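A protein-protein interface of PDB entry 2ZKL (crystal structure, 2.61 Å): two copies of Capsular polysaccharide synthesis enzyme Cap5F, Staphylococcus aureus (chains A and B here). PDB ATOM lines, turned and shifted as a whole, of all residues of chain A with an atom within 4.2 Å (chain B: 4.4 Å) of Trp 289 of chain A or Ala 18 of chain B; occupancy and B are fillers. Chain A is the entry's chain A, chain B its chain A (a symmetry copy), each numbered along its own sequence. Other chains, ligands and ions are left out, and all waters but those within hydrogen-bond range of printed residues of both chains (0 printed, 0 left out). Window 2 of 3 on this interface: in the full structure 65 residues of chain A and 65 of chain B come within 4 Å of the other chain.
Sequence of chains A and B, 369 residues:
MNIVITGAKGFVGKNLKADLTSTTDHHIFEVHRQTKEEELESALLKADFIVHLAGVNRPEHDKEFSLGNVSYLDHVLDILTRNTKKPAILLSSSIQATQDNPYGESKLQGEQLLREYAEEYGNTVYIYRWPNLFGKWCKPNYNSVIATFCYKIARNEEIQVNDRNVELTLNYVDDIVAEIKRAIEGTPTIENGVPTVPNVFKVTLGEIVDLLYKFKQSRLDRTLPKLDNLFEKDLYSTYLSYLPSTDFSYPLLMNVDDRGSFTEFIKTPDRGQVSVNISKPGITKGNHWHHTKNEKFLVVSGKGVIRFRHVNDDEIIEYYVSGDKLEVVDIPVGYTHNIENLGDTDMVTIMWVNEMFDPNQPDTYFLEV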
ATOM      1  N   HIS A 288     -19.994 -10.657   2.968  1.00  0.00           N
ATOM      2  CA  HIS A 288     -19.435 -10.318   1.665  1.00  0.00           C
ATOM      3  C   HIS A 288     -18.440  -9.175   1.820  1.00  0.00           C
ATOM      4  O   HIS A 288     -18.419  -8.518   2.858  1.00  0.00           O
ATOM      5  CB  HIS A 288     -20.562  -9.941   0.680  1.00  0.00           C
ATOM      6  CG  HIS A 288     -21.424  -8.796   1.128  1.00  0.00           C
ATOM      7  ND1 HIS A 288     -22.752  -8.684   0.767  1.00  0.00           N
ATOM      8  CD2 HIS A 288     -21.144  -7.692   1.867  1.00  0.00           C
ATOM      9  CE1 HIS A 288     -23.252  -7.565   1.263  1.00  0.00           C
ATOM     10  NE2 HIS A 288     -22.297  -6.944   1.934  1.00  0.00           N
ATOM     11  N   TRP A 289     -17.587  -8.967   0.819  1.00  0.00           N
ATOM     12  CA  TRP A 289     -16.633  -7.863   0.868  1.00  0.00           C
ATOM     13  C   TRP A 289     -16.694  -7.041  -0.417  1.00  0.00           C
ATOM     14  O   TRP A 289     -17.365  -7.424  -1.381  1.00  0.00           O
ATOM     15  CB  TRP A 289     -15.200  -8.350   1.107  1.00  0.00           C
ATOM     16  CG  TRP A 289     -14.677  -9.334   0.098  1.00  0.00           C
ATOM     17  CD1 TRP A 289     -14.921 -10.676   0.062  1.00  0.00           C
ATOM     18  CD2 TRP A 289     -13.797  -9.056  -1.004  1.00  0.00           C
ATOM     19  NE1 TRP A 289     -14.247 -11.253  -0.986  1.00  0.00           N
ATOM     20  CE2 TRP A 289     -13.550 -10.286  -1.659  1.00  0.00           C
ATOM     21  CE3 TRP A 289     -13.196  -7.890  -1.501  1.00  0.00           C
ATOM     22  CZ2 TRP A 289     -12.725 -10.386  -2.789  1.00  0.00           C
ATOM     23  CZ3 TRP A 289     -12.375  -7.985  -2.624  1.00  0.00           C
ATOM     24  CH2 TRP A 289     -12.148  -9.229  -3.257  1.00  0.00           C
ATOM     25  N   HIS A 290     -16.000  -5.903  -0.421  1.00  0.00           N
ATOM     26  CA  HIS A 290     -15.992  -5.031  -1.583  1.00  0.00           C
ATOM     27  C   HIS A 290     -14.579  -4.596  -1.897  1.00  0.00           C
ATOM     28  O   HIS A 290     -13.709  -4.620  -1.026  1.00  0.00           O
ATOM     29  CB  HIS A 290     -16.816  -3.769  -1.313  1.00  0.00           C
ATOM     30  CG  HIS A 290     -18.127  -4.024  -0.641  1.00  0.00           C
ATOM     31  ND1 HIS A 290     -19.231  -4.503  -1.312  1.00  0.00           N
ATOM     32  CD2 HIS A 290     -18.518  -3.836   0.640  1.00  0.00           C
ATOM     33  CE1 HIS A 290     -20.248  -4.594  -0.473  1.00  0.00           C
ATOM     34  NE2 HIS A 290     -19.839  -4.195   0.718  1.00  0.00           N
ATOM     35  N   HIS A 291     -14.360  -4.192  -3.144  1.00  0.00           N
ATOM     36  CA  HIS A 291     -13.056  -3.694  -3.564  1.00  0.00           C
ATOM     37  C   HIS A 291     -12.945  -2.225  -3.187  1.00  0.00           C
ATOM     38  O   HIS A 291     -11.944  -1.822  -2.601  1.00  0.00           O
ATOM     39  CB  HIS A 291     -12.862  -3.845  -5.074  1.00  0.00           C
ATOM     40  CG  HIS A 291     -12.124  -5.083  -5.460  1.00  0.00           C
ATOM     41  ND1 HIS A 291     -12.554  -5.926  -6.460  1.00  0.00           N
ATOM     42  CD2 HIS A 291     -10.985  -5.627  -4.970  1.00  0.00           C
ATOM     43  CE1 HIS A 291     -11.713  -6.938  -6.570  1.00  0.00           C
ATOM     44  NE2 HIS A 291     -10.752  -6.780  -5.676  1.00  0.00           N
ATOM     45  N   VAL A 311      -9.967 -10.361   4.122  1.00  0.00           N
ATOM     46  CA  VAL A 311      -9.990 -11.441   3.141  1.00  0.00           C
ATOM     47  C   VAL A 311      -8.804 -12.415   3.269  1.00  0.00           C
ATOM     48  O   VAL A 311      -8.997 -13.635   3.250  1.00  0.00           O
ATOM     49  CB  VAL A 311     -10.043 -10.862   1.701  1.00  0.00           C
ATOM     50  CG1 VAL A 311      -9.869 -11.968   0.676  1.00  0.00           C
ATOM     51  CG2 VAL A 311     -11.373 -10.171   1.480  1.00  0.00           C
ATOM     52  N   TYR A 335     -12.527  -6.265   3.761  1.00  0.00           N
ATOM     53  CA  TYR A 335     -12.929  -7.111   4.879  1.00  0.00           C
ATOM     54  C   TYR A 335     -14.333  -7.647   4.615  1.00  0.00           C
ATOM     55  O   TYR A 335     -15.227  -6.873   4.274  1.00  0.00           O
ATOM     56  CB  TYR A 335     -12.977  -6.332   6.205  1.00  0.00           C
ATOM     57  CG  TYR A 335     -11.654  -5.837   6.745  1.00  0.00           C
ATOM     58  CD1 TYR A 335     -11.037  -4.706   6.208  1.00  0.00           C
ATOM     59  CD2 TYR A 335     -11.023  -6.493   7.806  1.00  0.00           C
ATOM     60  CE1 TYR A 335      -9.818  -4.235   6.718  1.00  0.00           C
ATOM     61  CE2 TYR A 335      -9.801  -6.037   8.321  1.00  0.00           C
ATOM     62  CZ  TYR A 335      -9.204  -4.910   7.771  1.00  0.00           C
ATOM     63  OH  TYR A 335      -7.985  -4.461   8.245  1.00  0.00           O
ATOM     64  N   THR A 336     -14.548  -8.955   4.725  1.00  0.00           N
ATOM     65  CA  THR A 336     -15.921  -9.421   4.569  1.00  0.00           C
ATOM     66  C   THR A 336     -16.543  -8.974   5.872  1.00  0.00           C
ATOM     67  O   THR A 336     -15.855  -8.847   6.891  1.00  0.00           O
ATOM     68  CB  THR A 336     -16.073 -10.945   4.499  1.00  0.00           C
ATOM     69  OG1 THR A 336     -15.053 -11.579   5.286  1.00  0.00           O
ATOM     70  CG2 THR A 336     -16.018 -11.404   3.076  1.00  0.00           C
ATOM     71  N   ASP A 363     -19.918  -4.601  -6.598  1.00  0.00           N
ATOM     72  CA  ASP A 363     -18.571  -4.613  -6.089  1.00  0.00           C
ATOM     73  C   ASP A 363     -18.710  -5.286  -4.749  1.00  0.00           C
ATOM     74  O   ASP A 363     -18.217  -4.807  -3.734  1.00  0.00           O
ATOM     75  CB  ASP A 363     -18.028  -3.195  -5.950  1.00  0.00           C
ATOM     76  CG  ASP A 363     -16.642  -3.170  -5.371  1.00  0.00           C
ATOM     77  OD1 ASP A 363     -15.880  -4.114  -5.645  1.00  0.00           O
ATOM     78  OD2 ASP A 363     -16.306  -2.209  -4.650  1.00  0.00           O
ATOM     79  N   THR A 364     -19.430  -6.400  -4.760  1.00  0.00           N
ATOM     80  CA  THR A 364     -19.659  -7.168  -3.550  1.00  0.00           C
ATOM     81  C   THR A 364     -19.423  -8.642  -3.894  1.00  0.00           C
ATOM     82  O   THR A 364     -19.874  -9.129  -4.929  1.00  0.00           O
ATOM     83  CB  THR A 364     -21.095  -6.936  -3.013  1.00  0.00           C
ATOM     84  OG1 THR A 364     -21.995  -7.845  -3.640  1.00  0.00           O
ATOM     85  CG2 THR A 364     -21.561  -5.524  -3.337  1.00  0.00           C
ATOM     86  N   TYR A 365     -18.696  -9.341  -3.032  1.00  0.00           N
ATOM     87  CA  TYR A 365     -18.364 -10.744  -3.269  1.00  0.00           C
ATOM     88  C   TYR A 365     -18.634 -11.596  -2.033  1.00  0.00           C
ATOM     89  O   TYR A 365     -18.138 -11.301  -0.945  1.00  0.00           O
ATOM     90  CB  TYR A 365     -16.894 -10.836  -3.664  1.00  0.00           C
ATOM     91  CG  TYR A 365     -16.507  -9.744  -4.626  1.00  0.00           C
ATOM     92  CD1 TYR A 365     -17.045  -9.706  -5.914  1.00  0.00           C
ATOM     93  CD2 TYR A 365     -15.659  -8.706  -4.232  1.00  0.00           C
ATOM     94  CE1 TYR A 365     -16.753  -8.658  -6.793  1.00  0.00           C
ATOM     95  CE2 TYR A 365     -15.358  -7.651  -5.105  1.00  0.00           C
ATOM     96  CZ  TYR A 365     -15.914  -7.635  -6.381  1.00  0.00           C
ATOM     97  OH  TYR A 365     -15.656  -6.592  -7.240  1.00  0.00           O
ATOM     98  N   LEU A 367     -18.548 -14.225   0.874  1.00  0.00           N
ATOM     99  CA  LEU A 367     -17.483 -14.850   1.648  1.00  0.00           C
ATOM    100  C   LEU A 367     -17.910 -14.853   3.112  1.00  0.00           C
ATOM    101  O   LEU A 367     -17.919 -13.819   3.774  1.00  0.00           O
ATOM    102  CB  LEU A 367     -16.164 -14.091   1.470  1.00  0.00           C
ATOM    103  CG  LEU A 367     -14.961 -14.607   2.264  1.00  0.00           C
ATOM    104  CD1 LEU A 367     -14.602 -16.014   1.808  1.00  0.00           C
ATOM    105  CD2 LEU A 367     -13.776 -13.675   2.068  1.00  0.00           C
ATOM    106  N   LYS B  14      -2.166 -10.132  -4.762  1.00  0.00           N
ATOM    107  CA  LYS B  14      -3.208 -10.487  -3.803  1.00  0.00           C
ATOM    108  C   LYS B  14      -4.568  -9.977  -4.269  1.00  0.00           C
ATOM    109  O   LYS B  14      -5.584 -10.655  -4.109  1.00  0.00           O
ATOM    110  CB  LYS B  14      -2.892  -9.919  -2.416  1.00  0.00           C
ATOM    111  CG  LYS B  14      -1.465 -10.138  -1.906  1.00  0.00           C
ATOM    112  CD  LYS B  14      -1.452 -10.051  -0.381  1.00  0.00           C
ATOM    113  CE  LYS B  14      -0.152  -9.485   0.191  1.00  0.00           C
ATOM    114  NZ  LYS B  14      -0.062  -7.983   0.107  1.00  0.00           N
ATOM    115  N   ASN B  15      -4.582  -8.783  -4.852  1.00  0.00           N
ATOM    116  CA  ASN B  15      -5.820  -8.207  -5.354  1.00  0.00           C
ATOM    117  C   ASN B  15      -6.373  -8.952  -6.548  1.00  0.00           C
ATOM    118  O   ASN B  15      -7.572  -9.231  -6.610  1.00  0.00           O
ATOM    119  CB  ASN B  15      -5.626  -6.742  -5.743  1.00  0.00           C
ATOM    120  CG  ASN B  15      -5.729  -5.815  -4.555  1.00  0.00           C
ATOM    121  OD1 ASN B  15      -4.724  -5.318  -4.040  1.00  0.00           O
ATOM    122  ND2 ASN B  15      -6.952  -5.591  -4.099  1.00  0.00           N
ATOM    123  N   LEU B  16      -5.510  -9.266  -7.508  1.00  0.00           N
ATOM    124  CA  LEU B  16      -5.962  -9.975  -8.697  1.00  0.00           C
ATOM    125  C   LEU B  16      -6.485 -11.340  -8.301  1.00  0.00           C
ATOM    126  O   LEU B  16      -7.537 -11.772  -8.765  1.00  0.00           O
ATOM    127  CB  LEU B  16      -4.818 -10.124  -9.700  1.00  0.00           C
ATOM    128  CG  LEU B  16      -5.138 -10.788 -11.046  1.00  0.00           C
ATOM    129  CD1 LEU B  16      -6.296 -10.065 -11.742  1.00  0.00           C
ATOM    130  CD2 LEU B  16      -3.891 -10.761 -11.919  1.00  0.00           C
ATOM    131  N   LYS B  17      -5.757 -12.008  -7.418  1.00  0.00           N
ATOM    132  CA  LYS B  17      -6.157 -13.332  -6.973  1.00  0.00           C
ATOM    133  C   LYS B  17      -7.525 -13.304  -6.296  1.00  0.00           C
ATOM    134  O   LYS B  17      -8.405 -14.106  -6.619  1.00  0.00           O
ATOM    135  CB  LYS B  17      -5.124 -13.907  -6.001  1.00  0.00           C
ATOM    136  CG  LYS B  17      -5.482 -15.304  -5.543  1.00  0.00           C
ATOM    137  CD  LYS B  17      -5.044 -15.564  -4.118  1.00  0.00           C
ATOM    138  CE  LYS B  17      -5.764 -16.792  -3.559  1.00  0.00           C
ATOM    139  NZ  LYS B  17      -7.247 -16.659  -3.685  1.00  0.00           N
ATOM    140  N   ALA B  18      -7.694 -12.384  -5.351  1.00  0.00           N
ATOM    141  CA  ALA B  18      -8.953 -12.263  -4.621  1.00  0.00           C
ATOM    142  C   ALA B  18     -10.118 -12.068  -5.574  1.00  0.00           C
ATOM    143  O   ALA B  18     -11.148 -12.736  -5.453  1.00  0.00           O
ATOM    144  CB  ALA B  18      -8.884 -11.103  -3.638  1.00  0.00           C
ATOM    145  N   ASP B  19      -9.955 -11.157  -6.525  1.00  0.00           N
ATOM    146  CA  ASP B  19     -11.011 -10.891  -7.490  1.00  0.00           C
ATOM    147  C   ASP B  19     -11.301 -12.106  -8.370  1.00  0.00           C
ATOM    148  O   ASP B  19     -12.437 -12.589  -8.417  1.00  0.00           O
ATOM    149  CB  ASP B  19     -10.638  -9.693  -8.366  1.00  0.00           C
ATOM    150  CG  ASP B  19     -11.748  -9.299  -9.318  1.00  0.00           C
ATOM    151  OD1 ASP B  19     -12.046 -10.082 -10.246  1.00  0.00           O
ATOM    152  OD2 ASP B  19     -12.334  -8.208  -9.143  1.00  0.00           O
ATOM    153  N   LEU B  20     -10.267 -12.600  -9.054  1.00  0.00           N
ATOM    154  CA  LEU B  20     -10.394 -13.748  -9.952  1.00  0.00           C
ATOM    155  C   LEU B  20     -11.019 -14.988  -9.323  1.00  0.00           C
ATOM    156  O   LEU B  20     -11.843 -15.651  -9.950  1.00  0.00           O
ATOM    157  CB  LEU B  20      -9.028 -14.106 -10.546  1.00  0.00           C
ATOM    158  CG  LEU B  20      -8.760 -13.719 -12.007  1.00  0.00           C
ATOM    159  CD1 LEU B  20      -9.732 -12.653 -12.494  1.00  0.00           C
ATOM    160  CD2 LEU B  20      -7.331 -13.243 -12.125  1.00  0.00           C
ATOM    161  N   THR B  21     -10.638 -15.306  -8.090  1.00  0.00           N
ATOM    162  CA  THR B  21     -11.202 -16.482  -7.444  1.00  0.00           C
ATOM    163  C   THR B  21     -12.692 -16.313  -7.129  1.00  0.00           C
ATOM    164  O   THR B  21     -13.450 -17.284  -7.150  1.00  0.00           O
ATOM    165  CB  THR B  21     -10.436 -16.844  -6.141  1.00  0.00           C
ATOM    166  OG1 THR B  21     -10.512 -15.759  -5.209  1.00  0.00           O
ATOM    167  CG2 THR B  21      -8.972 -17.138  -6.446  1.00  0.00           C
ATOM    168  N   SER B  22     -13.118 -15.080  -6.865  1.00  0.00           N
ATOM    169  CA  SER B  22     -14.514 -14.807  -6.544  1.00  0.00           C
ATOM    170  C   SER B  22     -15.349 -14.478  -7.768  1.00  0.00           C
ATOM    171  O   SER B  22     -16.511 -14.853  -7.852  1.00  0.00           O
ATOM    172  CB  SER B  22     -14.616 -13.637  -5.563  1.00  0.00           C
ATOM    173  OG  SER B  22     -13.885 -13.889  -4.379  1.00  0.00           O
ATOM    174  N   TRP B 137      -4.167  -3.431  -0.492  1.00  0.00           N
ATOM    175  CA  TRP B 137      -3.176  -4.255   0.190  1.00  0.00           C
ATOM    176  C   TRP B 137      -1.688  -3.942   0.034  1.00  0.00           C
ATOM    177  O   TRP B 137      -0.836  -4.780   0.302  1.00  0.00           O
ATOM    178  CB  TRP B 137      -3.490  -5.723  -0.101  1.00  0.00           C
ATOM    179  CG  TRP B 137      -4.916  -6.032   0.289  1.00  0.00           C
ATOM    180  CD1 TRP B 137      -5.604  -5.487   1.334  1.00  0.00           C
ATOM    181  CD2 TRP B 137      -5.814  -6.960  -0.338  1.00  0.00           C
ATOM    182  NE1 TRP B 137      -6.868  -6.018   1.403  1.00  0.00           N
ATOM    183  CE2 TRP B 137      -7.024  -6.926   0.392  1.00  0.00           C
ATOM    184  CE3 TRP B 137      -5.710  -7.825  -1.438  1.00  0.00           C
ATOM    185  CZ2 TRP B 137      -8.129  -7.719   0.055  1.00  0.00           C
ATOM    186  CZ3 TRP B 137      -6.812  -8.616  -1.773  1.00  0.00           C
ATOM    187  CH2 TRP B 137      -8.003  -8.556  -1.024  1.00  0.00           C
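N of Tyr 365 of chain A lies within hydrogen-bond range of O of Trp 289 of chain A (2.9 Å).
N of His 291 of chain A is in hydrogen-bond range of OD1 of Asp 363 of chain A (2.9 Å).
A ring nitrogen (ND1) of His 291 of chain A lies within hydrogen-bond range of the side-chain hydroxyl (OH) of Tyr 365 of chain A (3.3 Å).
The backbone carbonyl oxygen (O) of Ala 18 of chain B is in hydrogen-bond range of the side-chain hydroxyl (OG1) of Thr 21 of chain B, 3.1 Å away.
The backbone carbonyl oxygen (O) of Ala 18 of chain B is in hydrogen-bond range of the side-chain hydroxyl (OG) of Ser 22 of chain B, 3.2 Å away.
CB of Ala 18 of chain B touches CH2 of Trp 289 of chain A, 3.8 Å away.
Asp 19 of chain B touches His 291 of chain A (OD2 to CE1, 2.9 Å).
Of the printed residues of chain B, Trp 289 of chain A touches Ala 18.
Of the printed residues of chain B, His 291 of chain A touches Asp 19.
Thr 364 of chain A touches none of the printed residues of chain B.
Ala 18 of chain B touches just one residue of chain A: Trp 289 (3.8 Å).
Of the printed residues of chain A, Asp 19 of chain B touches His 291.
Thr 21 of chain B touches none of the printed residues of chain A.
The nearest printed residue of chain A that does not touch Asp 19 of chain B is Tyr 365 of chain A (4.2 Å).
Of the 10 printed residues of chain B, 2 touch a printed residue of chain A.
Of the 11 printed residues of chain A, 2 touch a printed residue of chain B.
Hydrophobic or aromatic side chains of chain A that line the printed part of chain B: Trp 289 and His 291.
Among the printed residues, 2 pairs touch across the chains.
Among the printed residues, no Asp or Glu carboxylate lies within 4 Å of a Lys or Arg side-chain nitrogen of the other chain.
No position is printed for both chains.
Of the 2 pairs that touch across the chains among the printed residues, none has its exchanged pair printed and touching as well.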
